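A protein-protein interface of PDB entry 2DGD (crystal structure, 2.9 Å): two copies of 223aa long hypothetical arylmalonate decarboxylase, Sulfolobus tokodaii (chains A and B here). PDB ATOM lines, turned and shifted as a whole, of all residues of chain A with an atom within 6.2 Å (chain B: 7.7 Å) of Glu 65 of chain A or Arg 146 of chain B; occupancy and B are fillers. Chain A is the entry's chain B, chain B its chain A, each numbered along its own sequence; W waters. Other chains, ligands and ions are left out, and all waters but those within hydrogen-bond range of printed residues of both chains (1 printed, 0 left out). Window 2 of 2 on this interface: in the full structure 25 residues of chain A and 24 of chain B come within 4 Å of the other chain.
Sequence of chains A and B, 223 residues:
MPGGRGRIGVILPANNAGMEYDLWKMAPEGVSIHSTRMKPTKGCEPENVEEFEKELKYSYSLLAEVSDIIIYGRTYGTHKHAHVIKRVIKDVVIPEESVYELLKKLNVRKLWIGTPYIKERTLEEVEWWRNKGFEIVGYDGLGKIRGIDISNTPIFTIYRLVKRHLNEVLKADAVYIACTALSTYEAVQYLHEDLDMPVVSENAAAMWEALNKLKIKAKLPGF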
ATOM      1  N   ARG A   7      -7.127 -13.743   6.703  1.00  0.00           N
ATOM      2  CA  ARG A   7      -5.810 -13.120   6.677  1.00  0.00           C
ATOM      3  C   ARG A   7      -5.579 -12.507   5.312  1.00  0.00           C
ATOM      4  O   ARG A   7      -5.620 -13.194   4.298  1.00  0.00           O
ATOM      5  CB  ARG A   7      -4.726 -14.153   6.972  1.00  0.00           C
ATOM      6  CG  ARG A   7      -4.815 -14.759   8.357  1.00  0.00           C
ATOM      7  CD  ARG A   7      -3.432 -15.074   8.865  1.00  0.00           C
ATOM      8  NE  ARG A   7      -3.246 -16.476   9.219  1.00  0.00           N
ATOM      9  CZ  ARG A   7      -3.242 -16.938  10.462  1.00  0.00           C
ATOM     10  NH1 ARG A   7      -3.060 -18.222  10.686  1.00  0.00           N
ATOM     11  NH2 ARG A   7      -3.414 -16.114  11.486  1.00  0.00           N
ATOM     12  N   TYR A  60       5.548 -12.543  -3.539  1.00  0.00           N
ATOM     13  CA  TYR A  60       4.342 -13.337  -3.422  1.00  0.00           C
ATOM     14  C   TYR A  60       4.627 -14.600  -2.610  1.00  0.00           C
ATOM     15  O   TYR A  60       3.827 -14.999  -1.767  1.00  0.00           O
ATOM     16  CB  TYR A  60       3.829 -13.719  -4.812  1.00  0.00           C
ATOM     17  CG  TYR A  60       2.768 -14.794  -4.778  1.00  0.00           C
ATOM     18  CD1 TYR A  60       1.543 -14.571  -4.152  1.00  0.00           C
ATOM     19  CD2 TYR A  60       3.006 -16.048  -5.334  1.00  0.00           C
ATOM     20  CE1 TYR A  60       0.582 -15.572  -4.078  1.00  0.00           C
ATOM     21  CE2 TYR A  60       2.050 -17.059  -5.266  1.00  0.00           C
ATOM     22  CZ  TYR A  60       0.842 -16.816  -4.638  1.00  0.00           C
ATOM     23  OH  TYR A  60      -0.103 -17.817  -4.581  1.00  0.00           O
ATOM     24  N   SER A  61       5.772 -15.228  -2.857  1.00  0.00           N
ATOM     25  CA  SER A  61       6.118 -16.443  -2.144  1.00  0.00           C
ATOM     26  C   SER A  61       6.275 -16.194  -0.649  1.00  0.00           C
ATOM     27  O   SER A  61       6.155 -17.122   0.145  1.00  0.00           O
ATOM     28  CB  SER A  61       7.408 -17.040  -2.695  1.00  0.00           C
ATOM     29  OG  SER A  61       8.534 -16.286  -2.286  1.00  0.00           O
ATOM     30  N   LEU A  62       6.544 -14.948  -0.265  1.00  0.00           N
ATOM     31  CA  LEU A  62       6.709 -14.610   1.146  1.00  0.00           C
ATOM     32  C   LEU A  62       5.365 -14.430   1.859  1.00  0.00           C
ATOM     33  O   LEU A  62       5.293 -14.472   3.086  1.00  0.00           O
ATOM     34  CB  LEU A  62       7.524 -13.323   1.283  1.00  0.00           C
ATOM     35  CG  LEU A  62       8.980 -13.298   0.809  1.00  0.00           C
ATOM     36  CD1 LEU A  62       9.536 -11.905   1.010  1.00  0.00           C
ATOM     37  CD2 LEU A  62       9.809 -14.307   1.586  1.00  0.00           C
ATOM     38  N   LEU A  63       4.302 -14.246   1.081  1.00  0.00           N
ATOM     39  CA  LEU A  63       2.962 -14.021   1.617  1.00  0.00           C
ATOM     40  C   LEU A  63       1.979 -15.159   1.343  1.00  0.00           C
ATOM     41  O   LEU A  63       0.939 -15.262   1.990  1.00  0.00           O
ATOM     42  CB  LEU A  63       2.406 -12.721   1.018  1.00  0.00           C
ATOM     43  CG  LEU A  63       2.265 -11.436   1.839  1.00  0.00           C
ATOM     44  CD1 LEU A  63       3.286 -11.366   2.939  1.00  0.00           C
ATOM     45  CD2 LEU A  63       2.407 -10.257   0.905  1.00  0.00           C
ATOM     46  N   ALA A  64       2.319 -16.007   0.382  1.00  0.00           N
ATOM     47  CA  ALA A  64       1.467 -17.118  -0.039  1.00  0.00           C
ATOM     48  C   ALA A  64       0.876 -18.012   1.052  1.00  0.00           C
ATOM     49  O   ALA A  64      -0.300 -18.387   0.983  1.00  0.00           O
ATOM     50  CB  ALA A  64       2.222 -17.974  -1.042  1.00  0.00           C
ATOM     51  N   GLU A  65       1.681 -18.349   2.055  1.00  0.00           N
ATOM     52  CA  GLU A  65       1.248 -19.236   3.140  1.00  0.00           C
ATOM     53  C   GLU A  65       0.421 -18.598   4.259  1.00  0.00           C
ATOM     54  O   GLU A  65      -0.404 -19.267   4.867  1.00  0.00           O
ATOM     55  CB  GLU A  65       2.470 -19.922   3.754  1.00  0.00           C
ATOM     56  CG  GLU A  65       2.172 -20.918   4.850  1.00  0.00           C
ATOM     57  CD  GLU A  65       1.446 -22.151   4.336  1.00  0.00           C
ATOM     58  OE1 GLU A  65       1.815 -22.668   3.254  1.00  0.00           O
ATOM     59  OE2 GLU A  65       0.509 -22.613   5.026  1.00  0.00           O
ATOM     60  N   VAL A  66       0.647 -17.324   4.551  1.00  0.00           N
ATOM     61  CA  VAL A  66      -0.113 -16.670   5.607  1.00  0.00           C
ATOM     62  C   VAL A  66      -1.338 -15.947   5.069  1.00  0.00           C
ATOM     63  O   VAL A  66      -2.187 -15.504   5.841  1.00  0.00           O
ATOM     64  CB  VAL A  66       0.718 -15.609   6.367  1.00  0.00           C
ATOM     65  CG1 VAL A  66       1.925 -16.243   6.997  1.00  0.00           C
ATOM     66  CG2 VAL A  66       1.125 -14.494   5.426  1.00  0.00           C
ATOM     67  N   SER A  67      -1.438 -15.830   3.751  1.00  0.00           N
ATOM     68  CA  SER A  67      -2.549 -15.104   3.146  1.00  0.00           C
ATOM     69  C   SER A  67      -3.709 -15.932   2.615  1.00  0.00           C
ATOM     70  O   SER A  67      -3.515 -17.019   2.065  1.00  0.00           O
ATOM     71  CB  SER A  67      -2.025 -14.223   2.009  1.00  0.00           C
ATOM     72  OG  SER A  67      -1.021 -13.335   2.464  1.00  0.00           O
ATOM     73  N   ALA B  14       8.703 -15.051   6.647  1.00  0.00           N
ATOM     74  CA  ALA B  14       7.555 -15.145   5.763  1.00  0.00           C
ATOM     75  C   ALA B  14       6.300 -15.725   6.396  1.00  0.00           C
ATOM     76  O   ALA B  14       5.214 -15.167   6.259  1.00  0.00           O
ATOM     77  CB  ALA B  14       7.924 -15.955   4.517  1.00  0.00           C
ATOM     78  N   ASN B  15       6.448 -16.841   7.097  1.00  0.00           N
ATOM     79  CA  ASN B  15       5.298 -17.507   7.687  1.00  0.00           C
ATOM     80  C   ASN B  15       4.903 -17.137   9.108  1.00  0.00           C
ATOM     81  O   ASN B  15       4.177 -17.877   9.761  1.00  0.00           O
ATOM     82  CB  ASN B  15       5.489 -19.014   7.572  1.00  0.00           C
ATOM     83  CG  ASN B  15       5.601 -19.463   6.134  1.00  0.00           C
ATOM     84  OD1 ASN B  15       4.743 -19.144   5.308  1.00  0.00           O
ATOM     85  ND2 ASN B  15       6.661 -20.198   5.819  1.00  0.00           N
ATOM     86  N   ASN B  16       5.369 -15.993   9.587  1.00  0.00           N
ATOM     87  CA  ASN B  16       5.009 -15.550  10.923  1.00  0.00           C
ATOM     88  C   ASN B  16       3.691 -14.788  10.802  1.00  0.00           C
ATOM     89  O   ASN B  16       3.638 -13.735  10.167  1.00  0.00           O
ATOM     90  CB  ASN B  16       6.087 -14.623  11.486  1.00  0.00           C
ATOM     91  CG  ASN B  16       5.756 -14.127  12.882  1.00  0.00           C
ATOM     92  OD1 ASN B  16       4.653 -13.642  13.140  1.00  0.00           O
ATOM     93  ND2 ASN B  16       6.717 -14.241  13.790  1.00  0.00           N
ATOM     94  N   ALA B  17       2.628 -15.306  11.405  1.00  0.00           N
ATOM     95  CA  ALA B  17       1.339 -14.635  11.317  1.00  0.00           C
ATOM     96  C   ALA B  17       0.848 -14.093  12.651  1.00  0.00           C
ATOM     97  O   ALA B  17      -0.270 -13.595  12.747  1.00  0.00           O
ATOM     98  CB  ALA B  17       0.299 -15.578  10.730  1.00  0.00           C
ATOM     99  N   PRO B 116       6.894 -22.988  21.808  1.00  0.00           N
ATOM    100  CA  PRO B 116       5.975 -23.685  20.912  1.00  0.00           C
ATOM    101  C   PRO B 116       6.696 -24.853  20.231  1.00  0.00           C
ATOM    102  O   PRO B 116       6.090 -25.624  19.494  1.00  0.00           O
ATOM    103  CB  PRO B 116       5.591 -22.592  19.928  1.00  0.00           C
ATOM    104  CG  PRO B 116       6.888 -21.886  19.736  1.00  0.00           C
ATOM    105  CD  PRO B 116       7.471 -21.803  21.146  1.00  0.00           C
ATOM    106  N   GLY B 143       5.412 -28.380  21.039  1.00  0.00           N
ATOM    107  CA  GLY B 143       5.872 -29.396  20.110  1.00  0.00           C
ATOM    108  C   GLY B 143       5.455 -29.173  18.674  1.00  0.00           C
ATOM    109  O   GLY B 143       4.972 -30.099  18.024  1.00  0.00           O
ATOM    110  N   LYS B 144       5.624 -27.950  18.174  1.00  0.00           N
ATOM    111  CA  LYS B 144       5.269 -27.633  16.792  1.00  0.00           C
ATOM    112  C   LYS B 144       6.540 -27.351  16.015  1.00  0.00           C
ATOM    113  O   LYS B 144       7.595 -27.107  16.605  1.00  0.00           O
ATOM    114  CB  LYS B 144       4.336 -26.419  16.724  1.00  0.00           C
ATOM    115  CG  LYS B 144       2.945 -26.682  17.262  1.00  0.00           C
ATOM    116  CD  LYS B 144       2.020 -25.500  17.036  1.00  0.00           C
ATOM    117  CE  LYS B 144       0.616 -25.792  17.554  1.00  0.00           C
ATOM    118  NZ  LYS B 144      -0.315 -24.648  17.331  1.00  0.00           N
ATOM    119  N   ILE B 145       6.440 -27.381  14.691  1.00  0.00           N
ATOM    120  CA  ILE B 145       7.600 -27.151  13.842  1.00  0.00           C
ATOM    121  C   ILE B 145       7.405 -26.017  12.844  1.00  0.00           C
ATOM    122  O   ILE B 145       8.251 -25.134  12.732  1.00  0.00           O
ATOM    123  CB  ILE B 145       7.955 -28.426  13.065  1.00  0.00           C
ATOM    124  CG1 ILE B 145       8.217 -29.571  14.039  1.00  0.00           C
ATOM    125  CG2 ILE B 145       9.172 -28.182  12.201  1.00  0.00           C
ATOM    126  CD1 ILE B 145       8.388 -30.911  13.359  1.00  0.00           C
ATOM    127  N   ARG B 146       6.294 -26.053  12.121  1.00  0.00           N
ATOM    128  CA  ARG B 146       5.987 -25.042  11.120  1.00  0.00           C
ATOM    129  C   ARG B 146       5.494 -23.740  11.742  1.00  0.00           C
ATOM    130  O   ARG B 146       4.622 -23.742  12.609  1.00  0.00           O
ATOM    131  CB  ARG B 146       4.944 -25.587  10.134  1.00  0.00           C
ATOM    132  CG  ARG B 146       5.473 -26.691   9.241  1.00  0.00           C
ATOM    133  CD  ARG B 146       4.367 -27.469   8.552  1.00  0.00           C
ATOM    134  NE  ARG B 146       3.555 -26.663   7.643  1.00  0.00           N
ATOM    135  CZ  ARG B 146       2.358 -26.170   7.945  1.00  0.00           C
ATOM    136  NH1 ARG B 146       1.697 -25.457   7.051  1.00  0.00           N
ATOM    137  NH2 ARG B 146       1.822 -26.384   9.139  1.00  0.00           N
ATOM    138  N   GLY B 147       6.060 -22.628  11.283  1.00  0.00           N
ATOM    139  CA  GLY B 147       5.685 -21.325  11.797  1.00  0.00           C
ATOM    140  C   GLY B 147       4.213 -20.989  11.673  1.00  0.00           C
ATOM    141  O   GLY B 147       3.635 -20.397  12.582  1.00  0.00           O
ATOM    142  N   ILE B 148       3.594 -21.356  10.556  1.00  0.00           N
ATOM    143  CA  ILE B 148       2.180 -21.064  10.372  1.00  0.00           C
ATOM    144  C   ILE B 148       1.366 -21.812  11.430  1.00  0.00           C
ATOM    145  O   ILE B 148       0.386 -21.294  11.961  1.00  0.00           O
ATOM    146  CB  ILE B 148       1.710 -21.465   8.957  1.00  0.00           C
ATOM    147  CG1 ILE B 148       0.569 -20.560   8.531  1.00  0.00           C
ATOM    148  CG2 ILE B 148       1.251 -22.890   8.925  1.00  0.00           C
ATOM    149  CD1 ILE B 148       1.008 -19.133   8.324  1.00  0.00           C
ATOM    150  N   ASP B 149       1.798 -23.029  11.743  1.00  0.00           N
ATOM    151  CA  ASP B 149       1.130 -23.847  12.741  1.00  0.00           C
ATOM    152  C   ASP B 149       1.290 -23.158  14.093  1.00  0.00           C
ATOM    153  O   ASP B 149       0.340 -23.056  14.870  1.00  0.00           O
ATOM    154  CB  ASP B 149       1.759 -25.243  12.780  1.00  0.00           C
ATOM    155  CG  ASP B 149       1.097 -26.158  13.797  1.00  0.00           C
ATOM    156  OD1 ASP B 149       1.702 -27.194  14.147  1.00  0.00           O
ATOM    157  OD2 ASP B 149      -0.026 -25.848  14.240  1.00  0.00           O
ATOM    158  N   ILE B 150       2.500 -22.682  14.364  1.00  0.00           N
ATOM    159  CA  ILE B 150       2.780 -21.992  15.612  1.00  0.00           C
ATOM    160  C   ILE B 150       1.895 -20.760  15.735  1.00  0.00           C
ATOM    161  O   ILE B 150       1.296 -20.525  16.785  1.00  0.00           O
ATOM    162  CB  ILE B 150       4.258 -21.570  15.680  1.00  0.00           C
ATOM    163  CG1 ILE B 150       5.137 -22.826  15.686  1.00  0.00           C
ATOM    164  CG2 ILE B 150       4.514 -20.721  16.915  1.00  0.00           C
ATOM    165  CD1 ILE B 150       6.610 -22.551  15.680  1.00  0.00           C
ATOM    166  N   SER B 151       1.805 -19.988  14.656  1.00  0.00           N
ATOM    167  CA  SER B 151       0.994 -18.775  14.629  1.00  0.00           C
ATOM    168  C   SER B 151      -0.473 -19.061  14.913  1.00  0.00           C
ATOM    169  O   SER B 151      -1.169 -18.241  15.523  1.00  0.00           O
ATOM    170  CB  SER B 151       1.105 -18.090  13.264  1.00  0.00           C
ATOM    171  OG  SER B 151       2.420 -17.635  13.009  1.00  0.00           O
ATOM    172  N   ASN B 152      -0.946 -20.220  14.469  1.00  0.00           N
ATOM    173  CA  ASN B 152      -2.338 -20.583  14.675  1.00  0.00           C
ATOM    174  C   ASN B 152      -2.702 -20.950  16.109  1.00  0.00           C
ATOM    175  O   ASN B 152      -3.864 -21.208  16.398  1.00  0.00           O
ATOM    176  CB  ASN B 152      -2.715 -21.741  13.754  1.00  0.00           C
ATOM    177  CG  ASN B 152      -2.645 -21.365  12.296  1.00  0.00           C
ATOM    178  OD1 ASN B 152      -2.963 -20.249  11.932  1.00  0.00           O
ATOM    179  ND2 ASN B 152      -2.242 -22.299  11.453  1.00  0.00           N
ATOM    180  N   THR B 153      -1.727 -20.968  17.012  1.00  0.00           N
ATOM    181  CA  THR B 153      -2.001 -21.341  18.392  1.00  0.00           C
ATOM    182  C   THR B 153      -2.990 -20.412  19.091  1.00  0.00           C
ATOM    183  O   THR B 153      -2.768 -19.200  19.193  1.00  0.00           O
ATOM    184  CB  THR B 153      -0.713 -21.392  19.209  1.00  0.00           C
ATOM    185  OG1 THR B 153       0.248 -22.201  18.522  1.00  0.00           O
ATOM    186  CG2 THR B 153      -0.988 -21.983  20.596  1.00  0.00           C
ATOM    187  N   ALA B 181       6.270 -15.810  16.693  1.00  0.00           N
ATOM    188  CA  ALA B 181       5.185 -16.309  15.835  1.00  0.00           C
ATOM    189  C   ALA B 181       3.892 -16.496  16.643  1.00  0.00           C
ATOM    190  O   ALA B 181       2.796 -16.506  16.089  1.00  0.00           O
ATOM    191  CB  ALA B 181       5.582 -17.615  15.186  1.00  0.00           C
HETATM  192  O   HOH W   1      -0.417 -25.118   5.187  1.00  0.00           O
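No residue of chain B comes within 4 Å of Ala 64 of chain A.
Glu 65 of chain A touches just these residues of chain B: Asn 15, Arg 146 and Ile 148.
Printed residues of chain A within 4 Å of Asn 15 of chain B: Glu 65 (2.9 Å) and Val 66 (3.7 Å).
Of the printed residues of chain A, Ala 17 of chain B touches Arg 7 (3.8 Å).
Of chain A, only Glu 65 comes within 4 Å of Arg 146 of chain B.
The nearest residue of chain B that does not touch Glu 65 of chain A is Ala 14 of chain B (6.0 Å).
The nearest printed residue of chain A that does not touch Asn 15 of chain B is Leu 62 of chain A (4.8 Å).
No position is printed for both chains.
NH1 of Arg 146 of chain B is in salt-bridge range of OE2 of Glu 65 of chain A.
OD1 of Asn 152 of chain B sits close to NH1 of Arg 7 of chain A (2.4 Å).
O of Leu 62 of chain A sits close to O of Ala 14 of chain B.
Hydrophobic or aromatic side chains of chain A within 4 Å of the printed part of chain B: Leu 62 and Val 66.
Of the 17 printed residues of chain B, 6 touch a printed residue of chain A.
Hydrophobic or aromatic side chains of chain B that line the printed part of chain A: Ala 14, Ala 17 and Ile 148.
Ala 17 of chain B touches Arg 7 of chain A.
CB of Glu 65 of chain A touches OD1 of Asn 15 of chain B, 2.9 Å away.
CD1 of Ile 148 of chain B touches O of Glu 65 of chain A, 3.7 Å away.
Ala 14 of chain B touches Val 66 of chain A.
CG1 of Val 66 of chain A touches CA of Asn 15 of chain B, at 3.7 Å.
Ile 148 of chain B touches Val 66 of chain A (CD1 to CG1, 3.3 Å).
The backbone NH of Ala 17 of chain B is in hydrogen-bond range of the side-chain hydroxyl of Ser 151 of chain B, at 2.8 Å.
The backbone carbonyl oxygen (O) of Ile 148 of chain B lies within hydrogen-bond range of the side-chain amide nitrogen (ND2) of Asn 152 of chain B, 2.9 Å away.
Water W1 bridges the side-chain carboxylate of Glu 65 of chain A (2.7 Å) and the guanidinium group of Arg 146 of chain B (2.8 Å).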
